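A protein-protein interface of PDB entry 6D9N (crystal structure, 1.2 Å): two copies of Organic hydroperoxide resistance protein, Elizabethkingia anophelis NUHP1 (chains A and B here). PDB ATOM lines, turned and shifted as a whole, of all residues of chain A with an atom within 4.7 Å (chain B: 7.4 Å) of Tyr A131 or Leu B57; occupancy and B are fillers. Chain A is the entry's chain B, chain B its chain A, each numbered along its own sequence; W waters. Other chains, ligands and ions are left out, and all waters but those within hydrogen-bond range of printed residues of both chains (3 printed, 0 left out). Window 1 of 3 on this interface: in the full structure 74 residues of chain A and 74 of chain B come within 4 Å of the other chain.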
ATOM      1  N   LEU A  34     -33.646  24.899 -16.791  1.00  0.00           N
ATOM      2  CA  LEU A  34     -32.251  24.597 -16.491  1.00  0.00           C
ATOM      3  C   LEU A  34     -31.548  25.924 -16.182  1.00  0.00           C
ATOM      4  O   LEU A  34     -31.622  26.859 -16.984  1.00  0.00           O
ATOM      5  CB  LEU A  34     -31.612  23.889 -17.703  1.00  0.00           C
ATOM      6  CG  LEU A  34     -30.155  23.463 -17.736  1.00  0.00           C
ATOM      7  CD1 LEU A  34     -29.909  22.312 -18.747  1.00  0.00           C
ATOM      8  CD2 LEU A  34     -29.229  24.642 -18.088  1.00  0.00           C
ATOM      9  N   LEU A  57     -22.376  18.431 -19.554  1.00  0.00           N
ATOM     10  CA  LEU A  57     -23.664  18.618 -20.219  1.00  0.00           C
ATOM     11  C   LEU A  57     -23.765  17.737 -21.458  1.00  0.00           C
ATOM     12  O   LEU A  57     -24.850  17.231 -21.776  1.00  0.00           O
ATOM     13  CB  LEU A  57     -23.867  20.099 -20.568  1.00  0.00           C
ATOM     14  CG  LEU A  57     -24.166  20.993 -19.372  1.00  0.00           C
ATOM     15  CD1 LEU A  57     -23.934  22.475 -19.731  1.00  0.00           C
ATOM     16  CD2 LEU A  57     -25.564  20.768 -18.854  1.00  0.00           C
ATOM     17  N   PHE A  58     -22.658  17.554 -22.175  1.00  0.00           N
ATOM     18  CA  PHE A  58     -22.672  16.669 -23.330  1.00  0.00           C
ATOM     19  C   PHE A  58     -22.887  15.216 -22.935  1.00  0.00           C
ATOM     20  O   PHE A  58     -23.657  14.495 -23.593  1.00  0.00           O
ATOM     21  CB  PHE A  58     -21.371  16.823 -24.138  1.00  0.00           C
ATOM     22  CG  PHE A  58     -21.495  16.274 -25.544  1.00  0.00           C
ATOM     23  CD1 PHE A  58     -22.278  16.917 -26.499  1.00  0.00           C
ATOM     24  CD2 PHE A  58     -20.823  15.132 -25.924  1.00  0.00           C
ATOM     25  CE1 PHE A  58     -22.431  16.405 -27.794  1.00  0.00           C
ATOM     26  CE2 PHE A  58     -20.965  14.636 -27.233  1.00  0.00           C
ATOM     27  CZ  PHE A  58     -21.740  15.293 -28.147  1.00  0.00           C
ATOM     28  N   ALA A  60     -24.435  14.187 -20.188  1.00  0.00           N
ATOM     29  CA  ALA A  60     -25.814  14.101 -19.725  1.00  0.00           C
ATOM     30  C   ALA A  60     -26.783  14.085 -20.906  1.00  0.00           C
ATOM     31  O   ALA A  60     -27.704  13.243 -20.977  1.00  0.00           O
ATOM     32  CB  ALA A  60     -26.099  15.264 -18.786  1.00  0.00           C
ATOM     33  N   GLY A  61     -26.577  15.003 -21.855  1.00  0.00           N
ATOM     34  CA  GLY A  61     -27.462  15.068 -23.006  1.00  0.00           C
ATOM     35  C   GLY A  61     -27.375  13.829 -23.879  1.00  0.00           C
ATOM     36  O   GLY A  61     -28.399  13.355 -24.380  1.00  0.00           O
ATOM     37  N   TYR A  62     -26.157  13.331 -24.126  1.00  0.00           N
ATOM     38  CA  TYR A  62     -26.020  12.181 -25.011  1.00  0.00           C
ATOM     39  C   TYR A  62     -26.633  10.937 -24.361  1.00  0.00           C
ATOM     40  O   TYR A  62     -27.358  10.163 -25.007  1.00  0.00           O
ATOM     41  CB  TYR A  62     -24.553  11.969 -25.373  1.00  0.00           C
ATOM     42  CG  TYR A  62     -24.312  11.265 -26.705  1.00  0.00           C
ATOM     43  CD1 TYR A  62     -23.085  11.439 -27.375  1.00  0.00           C
ATOM     44  CD2 TYR A  62     -25.259  10.409 -27.296  1.00  0.00           C
ATOM     45  CE1 TYR A  62     -22.828  10.814 -28.584  1.00  0.00           C
ATOM     46  CE2 TYR A  62     -25.007   9.792 -28.527  1.00  0.00           C
ATOM     47  CZ  TYR A  62     -23.789   9.980 -29.137  1.00  0.00           C
ATOM     48  OH  TYR A  62     -23.480   9.351 -30.332  1.00  0.00           O
ATOM     49  N   CYS A  65     -30.346  11.371 -24.700  1.00  0.00           N
ATOM     50  CA  CYS A  65     -30.770  11.235 -26.088  1.00  0.00           C
ATOM     51  C   CYS A  65     -30.776   9.772 -26.493  1.00  0.00           C
ATOM     52  O   CYS A  65     -31.740   9.262 -27.089  1.00  0.00           O
ATOM     53  CB  CYS A  65     -29.777  12.022 -26.977  1.00  0.00           C
ATOM     54  SG  CYS A  65     -30.211  11.972 -28.757  1.00  0.00           S
ATOM     55  N   CYS A 129     -31.083   8.674 -32.568  1.00  0.00           N
ATOM     56  CA  CYS A 129     -30.555   9.691 -31.656  1.00  0.00           C
ATOM     57  C   CYS A 129     -29.928  10.877 -32.398  1.00  0.00           C
ATOM     58  O   CYS A 129     -28.909  10.698 -33.097  1.00  0.00           O
ATOM     59  CB  CYS A 129     -29.507   8.993 -30.788  1.00  0.00           C
ATOM     60  SG  CYS A 129     -28.557  10.013 -29.684  1.00  0.00           S
ATOM     61  N   PRO A 130     -30.425  12.098 -32.207  1.00  0.00           N
ATOM     62  CA  PRO A 130     -29.770  13.233 -32.882  1.00  0.00           C
ATOM     63  C   PRO A 130     -28.325  13.464 -32.501  1.00  0.00           C
ATOM     64  O   PRO A 130     -27.576  13.957 -33.354  1.00  0.00           O
ATOM     65  CB  PRO A 130     -30.648  14.436 -32.503  1.00  0.00           C
ATOM     66  CG  PRO A 130     -31.993  13.821 -32.405  1.00  0.00           C
ATOM     67  CD  PRO A 130     -31.772  12.442 -31.779  1.00  0.00           C
ATOM     68  N   TYR A 131     -27.903  13.133 -31.284  1.00  0.00           N
ATOM     69  CA  TYR A 131     -26.503  13.364 -30.938  1.00  0.00           C
ATOM     70  C   TYR A 131     -25.604  12.441 -31.735  1.00  0.00           C
ATOM     71  O   TYR A 131     -24.490  12.839 -32.135  1.00  0.00           O
ATOM     72  CB  TYR A 131     -26.240  13.117 -29.468  1.00  0.00           C
ATOM     73  CG  TYR A 131     -26.619  14.212 -28.470  1.00  0.00           C
ATOM     74  CD1 TYR A 131     -25.698  14.650 -27.541  1.00  0.00           C
ATOM     75  CD2 TYR A 131     -27.899  14.756 -28.426  1.00  0.00           C
ATOM     76  CE1 TYR A 131     -26.024  15.621 -26.574  1.00  0.00           C
ATOM     77  CE2 TYR A 131     -28.259  15.708 -27.484  1.00  0.00           C
ATOM     78  CZ  TYR A 131     -27.324  16.119 -26.532  1.00  0.00           C
ATOM     79  OH  TYR A 131     -27.655  17.041 -25.553  1.00  0.00           O
ATOM     80  N   SER A 132     -26.061  11.194 -31.979  1.00  0.00           N
ATOM     81  CA  SER A 132     -25.302  10.290 -32.836  1.00  0.00           C
ATOM     82  C   SER A 132     -25.232  10.806 -34.258  1.00  0.00           C
ATOM     83  O   SER A 132     -24.168  10.765 -34.886  1.00  0.00           O
ATOM     84  CB  SER A 132     -25.921   8.891 -32.826  1.00  0.00           C
ATOM     85  OG  SER A 132     -25.788   8.311 -31.550  1.00  0.00           O
ATOM     86  N   ASN A 133     -26.363  11.265 -34.811  1.00  0.00           N
ATOM     87  CA  ASN A 133     -26.321  11.820 -36.158  1.00  0.00           C
ATOM     88  C   ASN A 133     -25.458  13.069 -36.233  1.00  0.00           C
ATOM     89  O   ASN A 133     -24.794  13.285 -37.245  1.00  0.00           O
ATOM     90  CB  ASN A 133     -27.747  12.088 -36.635  1.00  0.00           C
ATOM     91  CG  ASN A 133     -28.502  10.791 -36.859  1.00  0.00           C
ATOM     92  OD1 ASN A 133     -27.982   9.886 -37.512  1.00  0.00           O
ATOM     93  ND2 ASN A 133     -29.715  10.684 -36.331  1.00  0.00           N
ATOM     94  N   ALA A 134     -25.421  13.872 -35.167  1.00  0.00           N
ATOM     95  CA  ALA A 134     -24.660  15.128 -35.216  1.00  0.00           C
ATOM     96  C   ALA A 134     -23.153  14.902 -35.180  1.00  0.00           C
ATOM     97  O   ALA A 134     -22.391  15.776 -35.615  1.00  0.00           O
ATOM     98  CB  ALA A 134     -25.071  16.008 -34.028  1.00  0.00           C
ATOM     99  N   THR A 135     -22.695  13.791 -34.604  1.00  0.00           N
ATOM    100  CA  THR A 135     -21.267  13.580 -34.348  1.00  0.00           C
ATOM    101  C   THR A 135     -20.614  12.566 -35.273  1.00  0.00           C
ATOM    102  O   THR A 135     -19.377  12.478 -35.288  1.00  0.00           O
ATOM    103  CB  THR A 135     -21.016  13.151 -32.887  1.00  0.00           C
ATOM    104  OG1 THR A 135     -21.747  11.958 -32.576  1.00  0.00           O
ATOM    105  CG2 THR A 135     -21.363  14.303 -31.928  1.00  0.00           C
ATOM    106  N   VAL B  27     -31.386  11.651 -15.212  1.00  0.00           N
ATOM    107  CA  VAL B  27     -29.988  11.719 -15.624  1.00  0.00           C
ATOM    108  C   VAL B  27     -29.146  12.173 -14.446  1.00  0.00           C
ATOM    109  O   VAL B  27     -29.553  13.082 -13.711  1.00  0.00           O
ATOM    110  CB  VAL B  27     -29.820  12.748 -16.751  1.00  0.00           C
ATOM    111  CG1 VAL B  27     -28.364  12.804 -17.182  1.00  0.00           C
ATOM    112  CG2 VAL B  27     -30.705  12.400 -17.915  1.00  0.00           C
ATOM    113  N   LEU B  34     -24.629  17.121 -11.423  1.00  0.00           N
ATOM    114  CA  LEU B  34     -25.839  17.327 -12.205  1.00  0.00           C
ATOM    115  C   LEU B  34     -26.750  16.135 -11.983  1.00  0.00           C
ATOM    116  O   LEU B  34     -26.338  14.984 -12.161  1.00  0.00           O
ATOM    117  CB  LEU B  34     -25.545  17.411 -13.698  1.00  0.00           C
ATOM    118  CG  LEU B  34     -25.094  18.750 -14.247  1.00  0.00           C
ATOM    119  CD1 LEU B  34     -25.040  18.667 -15.757  1.00  0.00           C
ATOM    120  CD2 LEU B  34     -26.030  19.853 -13.817  1.00  0.00           C
ATOM    121  N   PHE B  36     -31.097  15.378 -12.557  1.00  0.00           N
ATOM    122  CA  PHE B  36     -32.367  15.997 -12.905  1.00  0.00           C
ATOM    123  C   PHE B  36     -33.194  15.049 -13.752  1.00  0.00           C
ATOM    124  O   PHE B  36     -32.725  14.019 -14.226  1.00  0.00           O
ATOM    125  CB  PHE B  36     -32.092  17.297 -13.655  1.00  0.00           C
ATOM    126  CG  PHE B  36     -31.275  17.085 -14.897  1.00  0.00           C
ATOM    127  CD1 PHE B  36     -29.892  17.073 -14.837  1.00  0.00           C
ATOM    128  CD2 PHE B  36     -31.888  16.822 -16.101  1.00  0.00           C
ATOM    129  CE1 PHE B  36     -29.126  16.830 -15.987  1.00  0.00           C
ATOM    130  CE2 PHE B  36     -31.147  16.600 -17.240  1.00  0.00           C
ATOM    131  CZ  PHE B  36     -29.745  16.625 -17.188  1.00  0.00           C
ATOM    132  N   GLU B  37     -34.458  15.413 -13.895  1.00  0.00           N
ATOM    133  CA  GLU B  37     -35.399  14.606 -14.634  1.00  0.00           C
ATOM    134  C   GLU B  37     -35.559  15.152 -16.048  1.00  0.00           C
ATOM    135  O   GLU B  37     -35.404  16.354 -16.310  1.00  0.00           O
ATOM    136  CB  GLU B  37     -36.750  14.553 -13.921  1.00  0.00           C
ATOM    137  CG  GLU B  37     -36.702  13.850 -12.565  1.00  0.00           C
ATOM    138  CD  GLU B  37     -38.081  13.666 -11.995  1.00  0.00           C
ATOM    139  OE1 GLU B  37     -38.671  12.567 -12.150  1.00  0.00           O
ATOM    140  OE2 GLU B  37     -38.604  14.643 -11.429  1.00  0.00           O
ATOM    141  N   VAL B  38     -35.846  14.239 -16.977  1.00  0.00           N
ATOM    142  CA  VAL B  38     -36.103  14.598 -18.364  1.00  0.00           C
ATOM    143  C   VAL B  38     -37.445  14.012 -18.780  1.00  0.00           C
ATOM    144  O   VAL B  38     -37.841  12.927 -18.316  1.00  0.00           O
ATOM    145  CB  VAL B  38     -34.981  14.142 -19.317  1.00  0.00           C
ATOM    146  CG1 VAL B  38     -33.704  14.942 -19.049  1.00  0.00           C
ATOM    147  CG2 VAL B  38     -34.739  12.645 -19.238  1.00  0.00           C
ATOM    148  N   ALA B  52     -36.400  19.355 -18.381  1.00  0.00           N
ATOM    149  CA  ALA B  52     -35.302  19.312 -19.321  1.00  0.00           C
ATOM    150  C   ALA B  52     -35.524  18.198 -20.349  1.00  0.00           C
ATOM    151  O   ALA B  52     -36.379  17.317 -20.206  1.00  0.00           O
ATOM    152  CB  ALA B  52     -34.018  19.074 -18.541  1.00  0.00           C
ATOM    153  N   ASN B  53     -34.729  18.256 -21.399  1.00  0.00           N
ATOM    154  CA  ASN B  53     -34.709  17.242 -22.444  1.00  0.00           C
ATOM    155  C   ASN B  53     -33.346  17.322 -23.122  1.00  0.00           C
ATOM    156  O   ASN B  53     -32.548  18.235 -22.831  1.00  0.00           O
ATOM    157  CB  ASN B  53     -35.887  17.447 -23.428  1.00  0.00           C
ATOM    158  CG  ASN B  53     -35.908  18.847 -24.018  1.00  0.00           C
ATOM    159  OD1 ASN B  53     -34.910  19.328 -24.560  1.00  0.00           O
ATOM    160  ND2 ASN B  53     -37.048  19.511 -23.888  1.00  0.00           N
ATOM    161  N   PRO B  54     -33.008  16.360 -23.990  1.00  0.00           N
ATOM    162  CA  PRO B  54     -31.634  16.358 -24.535  1.00  0.00           C
ATOM    163  C   PRO B  54     -31.370  17.526 -25.459  1.00  0.00           C
ATOM    164  O   PRO B  54     -30.220  17.977 -25.568  1.00  0.00           O
ATOM    165  CB  PRO B  54     -31.508  14.978 -25.189  1.00  0.00           C
ATOM    166  CG  PRO B  54     -32.644  14.148 -24.589  1.00  0.00           C
ATOM    167  CD  PRO B  54     -33.738  15.110 -24.310  1.00  0.00           C
ATOM    168  N   GLU B  55     -32.403  18.071 -26.102  1.00  0.00           N
ATOM    169  CA  GLU B  55     -32.232  19.230 -26.966  1.00  0.00           C
ATOM    170  C   GLU B  55     -31.815  20.428 -26.127  1.00  0.00           C
ATOM    171  O   GLU B  55     -30.920  21.205 -26.506  1.00  0.00           O
ATOM    172  CB  GLU B  55     -33.537  19.547 -27.708  1.00  0.00           C
ATOM    173  CG  GLU B  55     -34.054  18.479 -28.660  1.00  0.00           C
ATOM    174  CD  GLU B  55     -34.970  17.403 -28.040  1.00  0.00           C
ATOM    175  OE1 GLU B  55     -34.926  17.139 -26.828  1.00  0.00           O
ATOM    176  OE2 GLU B  55     -35.647  16.693 -28.844  1.00  0.00           O
ATOM    177  N   MET B  56     -32.451  20.585 -24.964  1.00  0.00           N
ATOM    178  CA  MET B  56     -32.125  21.663 -24.041  1.00  0.00           C
ATOM    179  C   MET B  56     -30.718  21.512 -23.460  1.00  0.00           C
ATOM    180  O   MET B  56     -29.984  22.507 -23.300  1.00  0.00           O
ATOM    181  CB  MET B  56     -33.173  21.684 -22.905  1.00  0.00           C
ATOM    182  CG  MET B  56     -33.021  22.918 -21.980  1.00  0.00           C
ATOM    183  SD  MET B  56     -34.089  22.815 -20.524  1.00  0.00           S
ATOM    184  CE  MET B  56     -35.727  22.916 -21.277  1.00  0.00           C
ATOM    185  N   LEU B  57     -30.319  20.279 -23.146  1.00  0.00           N
ATOM    186  CA  LEU B  57     -28.958  20.039 -22.692  1.00  0.00           C
ATOM    187  C   LEU B  57     -27.950  20.400 -23.776  1.00  0.00           C
ATOM    188  O   LEU B  57     -26.867  20.920 -23.471  1.00  0.00           O
ATOM    189  CB  LEU B  57     -28.803  18.582 -22.237  1.00  0.00           C
ATOM    190  CG  LEU B  57     -29.501  18.308 -20.898  1.00  0.00           C
ATOM    191  CD1 LEU B  57     -29.778  16.788 -20.726  1.00  0.00           C
ATOM    192  CD2 LEU B  57     -28.741  18.873 -19.713  1.00  0.00           C
ATOM    193  N   PHE B  58     -28.283  20.141 -25.048  1.00  0.00           N
ATOM    194  CA  PHE B  58     -27.376  20.495 -26.127  1.00  0.00           C
ATOM    195  C   PHE B  58     -27.278  22.017 -26.259  1.00  0.00           C
ATOM    196  O   PHE B  58     -26.185  22.562 -26.468  1.00  0.00           O
ATOM    197  CB  PHE B  58     -27.819  19.847 -27.445  1.00  0.00           C
ATOM    198  CG  PHE B  58     -26.795  19.918 -28.514  1.00  0.00           C
ATOM    199  CD1 PHE B  58     -25.667  19.110 -28.457  1.00  0.00           C
ATOM    200  CD2 PHE B  58     -26.901  20.799 -29.563  1.00  0.00           C
ATOM    201  CE1 PHE B  58     -24.672  19.208 -29.454  1.00  0.00           C
ATOM    202  CE2 PHE B  58     -25.950  20.860 -30.554  1.00  0.00           C
ATOM    203  CZ  PHE B  58     -24.839  20.074 -30.513  1.00  0.00           C
ATOM    204  N   ALA B  59     -28.416  22.715 -26.148  1.00  0.00           N
ATOM    205  CA  ALA B  59     -28.386  24.183 -26.213  1.00  0.00           C
ATOM    206  C   ALA B  59     -27.545  24.771 -25.077  1.00  0.00           C
ATOM    207  O   ALA B  59     -26.721  25.687 -25.279  1.00  0.00           O
ATOM    208  CB  ALA B  59     -29.800  24.732 -26.139  1.00  0.00           C
ATOM    209  N   ALA B  60     -27.730  24.266 -23.860  1.00  0.00           N
ATOM    210  CA  ALA B  60     -26.976  24.735 -22.699  1.00  0.00           C
ATOM    211  C   ALA B  60     -25.501  24.429 -22.885  1.00  0.00           C
ATOM    212  O   ALA B  60     -24.644  25.297 -22.662  1.00  0.00           O
ATOM    213  CB  ALA B  60     -27.522  24.043 -21.448  1.00  0.00           C
ATOM    214  N   GLY B  61     -25.187  23.195 -23.292  1.00  0.00           N
ATOM    215  CA  GLY B  61     -23.791  22.832 -23.452  1.00  0.00           C
ATOM    216  C   GLY B  61     -23.092  23.586 -24.576  1.00  0.00           C
ATOM    217  O   GLY B  61     -21.938  23.993 -24.430  1.00  0.00           O
ATOM    218  N   TYR B  62     -23.772  23.790 -25.697  1.00  0.00           N
ATOM    219  CA  TYR B  62     -23.139  24.445 -26.825  1.00  0.00           C
ATOM    220  C   TYR B  62     -22.915  25.924 -26.498  1.00  0.00           C
ATOM    221  O   TYR B  62     -21.854  26.496 -26.774  1.00  0.00           O
ATOM    222  CB  TYR B  62     -23.980  24.264 -28.095  1.00  0.00           C
ATOM    223  CG  TYR B  62     -23.212  24.435 -29.408  1.00  0.00           C
ATOM    224  CD1 TYR B  62     -23.732  23.953 -30.584  1.00  0.00           C
ATOM    225  CD2 TYR B  62     -21.924  25.003 -29.476  1.00  0.00           C
ATOM    226  CE1 TYR B  62     -23.087  24.060 -31.795  1.00  0.00           C
ATOM    227  CE2 TYR B  62     -21.254  25.097 -30.697  1.00  0.00           C
ATOM    228  CZ  TYR B  62     -21.836  24.641 -31.843  1.00  0.00           C
ATOM    229  OH  TYR B  62     -21.194  24.719 -33.055  1.00  0.00           O
ATOM    230  N   SER B  63     -23.938  26.580 -25.940  1.00  0.00           N
ATOM    231  CA  SER B  63     -23.765  27.997 -25.595  1.00  0.00           C
ATOM    232  C   SER B  63     -22.602  28.174 -24.623  1.00  0.00           C
ATOM    233  O   SER B  63     -21.769  29.078 -24.783  1.00  0.00           O
ATOM    234  CB  SER B  63     -25.065  28.617 -25.071  1.00  0.00           C
ATOM    235  OG  SER B  63     -25.501  28.039 -23.852  1.00  0.00           O
ATOM    236  N   VAL B  90     -31.703  25.403 -30.429  1.00  0.00           N
ATOM    237  CA  VAL B  90     -31.532  24.049 -30.978  1.00  0.00           C
ATOM    238  C   VAL B  90     -32.882  23.531 -31.428  1.00  0.00           C
ATOM    239  O   VAL B  90     -33.803  23.452 -30.613  1.00  0.00           O
ATOM    240  CB  VAL B  90     -30.914  23.123 -29.928  1.00  0.00           C
ATOM    241  CG1 VAL B  90     -30.845  21.690 -30.446  1.00  0.00           C
ATOM    242  CG2 VAL B  90     -29.502  23.636 -29.544  1.00  0.00           C
ATOM    243  N   PHE B 100     -33.634  11.310 -36.305  1.00  0.00           N
ATOM    244  CA  PHE B 100     -33.837  12.723 -36.016  1.00  0.00           C
ATOM    245  C   PHE B 100     -32.508  13.451 -35.976  1.00  0.00           C
ATOM    246  O   PHE B 100     -31.476  12.867 -35.634  1.00  0.00           O
ATOM    247  CB  PHE B 100     -34.620  12.905 -34.696  1.00  0.00           C
ATOM    248  CG  PHE B 100     -35.975  12.275 -34.770  1.00  0.00           C
ATOM    249  CD1 PHE B 100     -36.166  10.956 -34.393  1.00  0.00           C
ATOM    250  CD2 PHE B 100     -37.045  12.977 -35.304  1.00  0.00           C
ATOM    251  CE1 PHE B 100     -37.397  10.342 -34.530  1.00  0.00           C
ATOM    252  CE2 PHE B 100     -38.293  12.373 -35.434  1.00  0.00           C
ATOM    253  CZ  PHE B 100     -38.462  11.053 -35.057  1.00  0.00           C
ATOM    254  N   GLY B 101     -32.543  14.725 -36.375  1.00  0.00           N
ATOM    255  CA  GLY B 101     -31.342  15.537 -36.430  1.00  0.00           C
ATOM    256  C   GLY B 101     -31.581  16.900 -35.813  1.00  0.00           C
ATOM    257  O   GLY B 101     -32.712  17.375 -35.679  1.00  0.00           O
ATOM    258  N   LEU B 102     -30.464  17.541 -35.437  1.00  0.00           N
ATOM    259  CA  LEU B 102     -30.463  18.883 -34.867  1.00  0.00           C
ATOM    260  C   LEU B 102     -30.120  19.946 -35.894  1.00  0.00           C
ATOM    261  O   LEU B 102     -29.550  19.676 -36.955  1.00  0.00           O
ATOM    262  CB  LEU B 102     -29.444  18.965 -33.711  1.00  0.00           C
ATOM    263  CG  LEU B 102     -29.669  17.928 -32.599  1.00  0.00           C
ATOM    264  CD1 LEU B 102     -28.635  18.142 -31.501  1.00  0.00           C
ATOM    265  CD2 LEU B 102     -31.112  17.979 -32.060  1.00  0.00           C
ATOM    266  N   TYR B 131     -17.767  21.434 -29.245  1.00  0.00           N
ATOM    267  CA  TYR B 131     -19.066  21.150 -29.844  1.00  0.00           C
ATOM    268  C   TYR B 131     -19.060  21.501 -31.322  1.00  0.00           C
ATOM    269  O   TYR B 131     -19.661  20.795 -32.139  1.00  0.00           O
ATOM    270  CB  TYR B 131     -20.205  21.891 -29.146  1.00  0.00           C
ATOM    271  CG  TYR B 131     -20.726  21.337 -27.849  1.00  0.00           C
ATOM    272  CD1 TYR B 131     -22.106  21.165 -27.670  1.00  0.00           C
ATOM    273  CD2 TYR B 131     -19.881  21.105 -26.729  1.00  0.00           C
ATOM    274  CE1 TYR B 131     -22.612  20.743 -26.443  1.00  0.00           C
ATOM    275  CE2 TYR B 131     -20.400  20.636 -25.508  1.00  0.00           C
ATOM    276  CZ  TYR B 131     -21.770  20.481 -25.372  1.00  0.00           C
ATOM    277  OH  TYR B 131     -22.322  20.091 -24.175  1.00  0.00           O
ATOM    278  N   ALA B 134     -17.074  18.839 -33.119  1.00  0.00           N
ATOM    279  CA  ALA B 134     -17.722  17.529 -33.119  1.00  0.00           C
ATOM    280  C   ALA B 134     -18.862  17.450 -34.130  1.00  0.00           C
ATOM    281  O   ALA B 134     -19.176  16.353 -34.632  1.00  0.00           O
ATOM    282  CB  ALA B 134     -18.280  17.192 -31.735  1.00  0.00           C
ATOM    283  N   THR B 135     -19.515  18.584 -34.436  1.00  0.00           N
ATOM    284  CA  THR B 135     -20.745  18.571 -35.229  1.00  0.00           C
ATOM    285  C   THR B 135     -20.554  19.137 -36.623  1.00  0.00           C
ATOM    286  O   THR B 135     -21.487  19.108 -37.424  1.00  0.00           O
ATOM    287  CB  THR B 135     -21.867  19.318 -34.501  1.00  0.00           C
ATOM    288  OG1 THR B 135     -21.507  20.693 -34.317  1.00  0.00           O
ATOM    289  CG2 THR B 135     -22.174  18.672 -33.148  1.00  0.00           C
ATOM    290  N   ASN B 138     -22.312  18.087 -40.106  1.00  0.00           N
ATOM    291  CA  ASN B 138     -23.403  17.148 -39.906  1.00  0.00           C
ATOM    292  C   ASN B 138     -24.711  17.828 -39.576  1.00  0.00           C
ATOM    293  O   ASN B 138     -25.768  17.211 -39.735  1.00  0.00           O
ATOM    294  CB  ASN B 138     -23.077  16.185 -38.758  1.00  0.00           C
ATOM    295  CG  ASN B 138     -22.043  15.153 -39.125  1.00  0.00           C
ATOM    296  OD1 ASN B 138     -21.997  14.685 -40.263  1.00  0.00           O
ATOM    297  ND2 ASN B 138     -21.269  14.726 -38.163  1.00  0.00           N
HETATM  298  O   HOH W   1     -27.425  15.362 -38.227  1.00  0.00           O
HETATM  299  O   HOH W   2     -28.199  15.755 -35.514  1.00  0.00           O
HETATM  300  O   HOH W   3     -24.431  12.560 -39.835  1.00  0.00           O
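O of Pro B54 is in hydrogen-bond range of OH of Tyr A131 (2.7 Å). The backbone carbonyl oxygen (O) of Ala A134 lies close to the backbone carbonyl oxygen (O) of Ala B134. N of Phe B58 is in hydrogen-bond range of OH of Tyr A131 (3.2 Å). The backbone NH of Phe A58 sits at hydrogen-bond distance from the side-chain hydroxyl of Tyr B131, 3.2 Å away. The side-chain amide nitrogen of Asn B138 lies within hydrogen-bond range of the backbone carbonyl oxygen of Ala A134 (3.0 Å). O of Phe B100 lies within hydrogen-bond range of ND2 of Asn A133 (2.9 Å).
The backbone NH (N) of Tyr A131 sits close to the side-chain sulfur (SG) of Cys A129. The backbone NH (N) of Val B27 lies within hydrogen-bond range of the backbone carbonyl oxygen (O) of Phe B36. O of Cys A129 lies within hydrogen-bond range of ND2 of Asn A133 (3.3 Å). O of Tyr A131 sits at hydrogen-bond distance from OG1 of Thr A135, 2.9 Å away. The backbone NH (N) of Met B56 sits at hydrogen-bond distance from the side-chain amide oxygen (OD1) of Asn B53 (2.8 Å). The side-chain sulfur of Cys A65 lies within hydrogen-bond range of the backbone NH of Tyr A131 (3.6 Å).
Among the printed residues, pairs that only touch across the chains: Pro A130 with Phe B100, Ala A134 with Thr B135, Thr A135 with Ala B134, Gly A61 with Pro B54, Pro A130 with Leu B102, Cys A65 with Pro B54, Thr A135 with Asn B138, Gly A61 with Leu B57, Asn A133 with Asn B138, Ala A60 with Val B27, Leu A57 with Gly B61, Leu A34 with Leu B57, Leu A57 with Leu B34, Leu A57 with Leu B57, Tyr A131 with Leu B57, Leu A34 with Ala B60, Leu A57 with Tyr B131, Leu A34 with Met B56 and Phe A58 with Phe B58.
Tyr A131 touches three residues of chain B. Printed residues of chain B within 4 Å of Asn A133: Phe B100 (2.9 Å) and Asn B138 (3.7 Å). Of the printed residues of chain A, Val B27 touches Ala A60 (3.7 Å). Of the printed residues of chain A, Leu B57 touches Leu A34 (3.8 Å), Leu A57 (3.8 Å), Gly A61 (3.7 Å) and Tyr A131 (3.8 Å). Of the printed residues of chain A, Phe B100 touches Pro A130 (3.3 Å) and Asn A133 (2.9 Å). The nearest residue of chain B that does not touch Tyr A131 is Leu B102 (4.6 Å).
Printed residues of chain A that touch a printed residue of chain B: Leu A34, Leu A57, Phe A58, Ala A60, Gly A61, Cys A65, Pro A130, Tyr A131, Asn A133, Ala A134 and Thr A135.
Leu A34 touches Ala B60, but with the chains exchanged Ala A60 does not touch Leu B34 (4.7 Å). Leu A57 touches Tyr B131, and with the chains exchanged Tyr A131 touches Leu B57. Phe A58 touches its own counterpart, Phe B58. Phe A58 touches Tyr B131, and with the chains exchanged Tyr A131 touches Phe B58. Positions printed for both chains: 34, 57, 58, 60, 61, 62, 131, 134 and 135.
Water W3 lies within hydrogen-bond range of the backbone carbonyl oxygen (O) of Asn A133 (2.7 Å) and the side-chain amide oxygen (OD1) of Asn B138 (3.3 Å). Water W2 lies within hydrogen-bond range of O of Pro A130 (2.9 Å), N of Leu B102 (2.9 Å) and N of Ala A134 (3.4 Å). Water W1 lies within hydrogen-bond range of the backbone carbonyl oxygen of Asn B138 (2.9 Å) and the backbone carbonyl oxygen of Asn A133 (3.5 Å).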
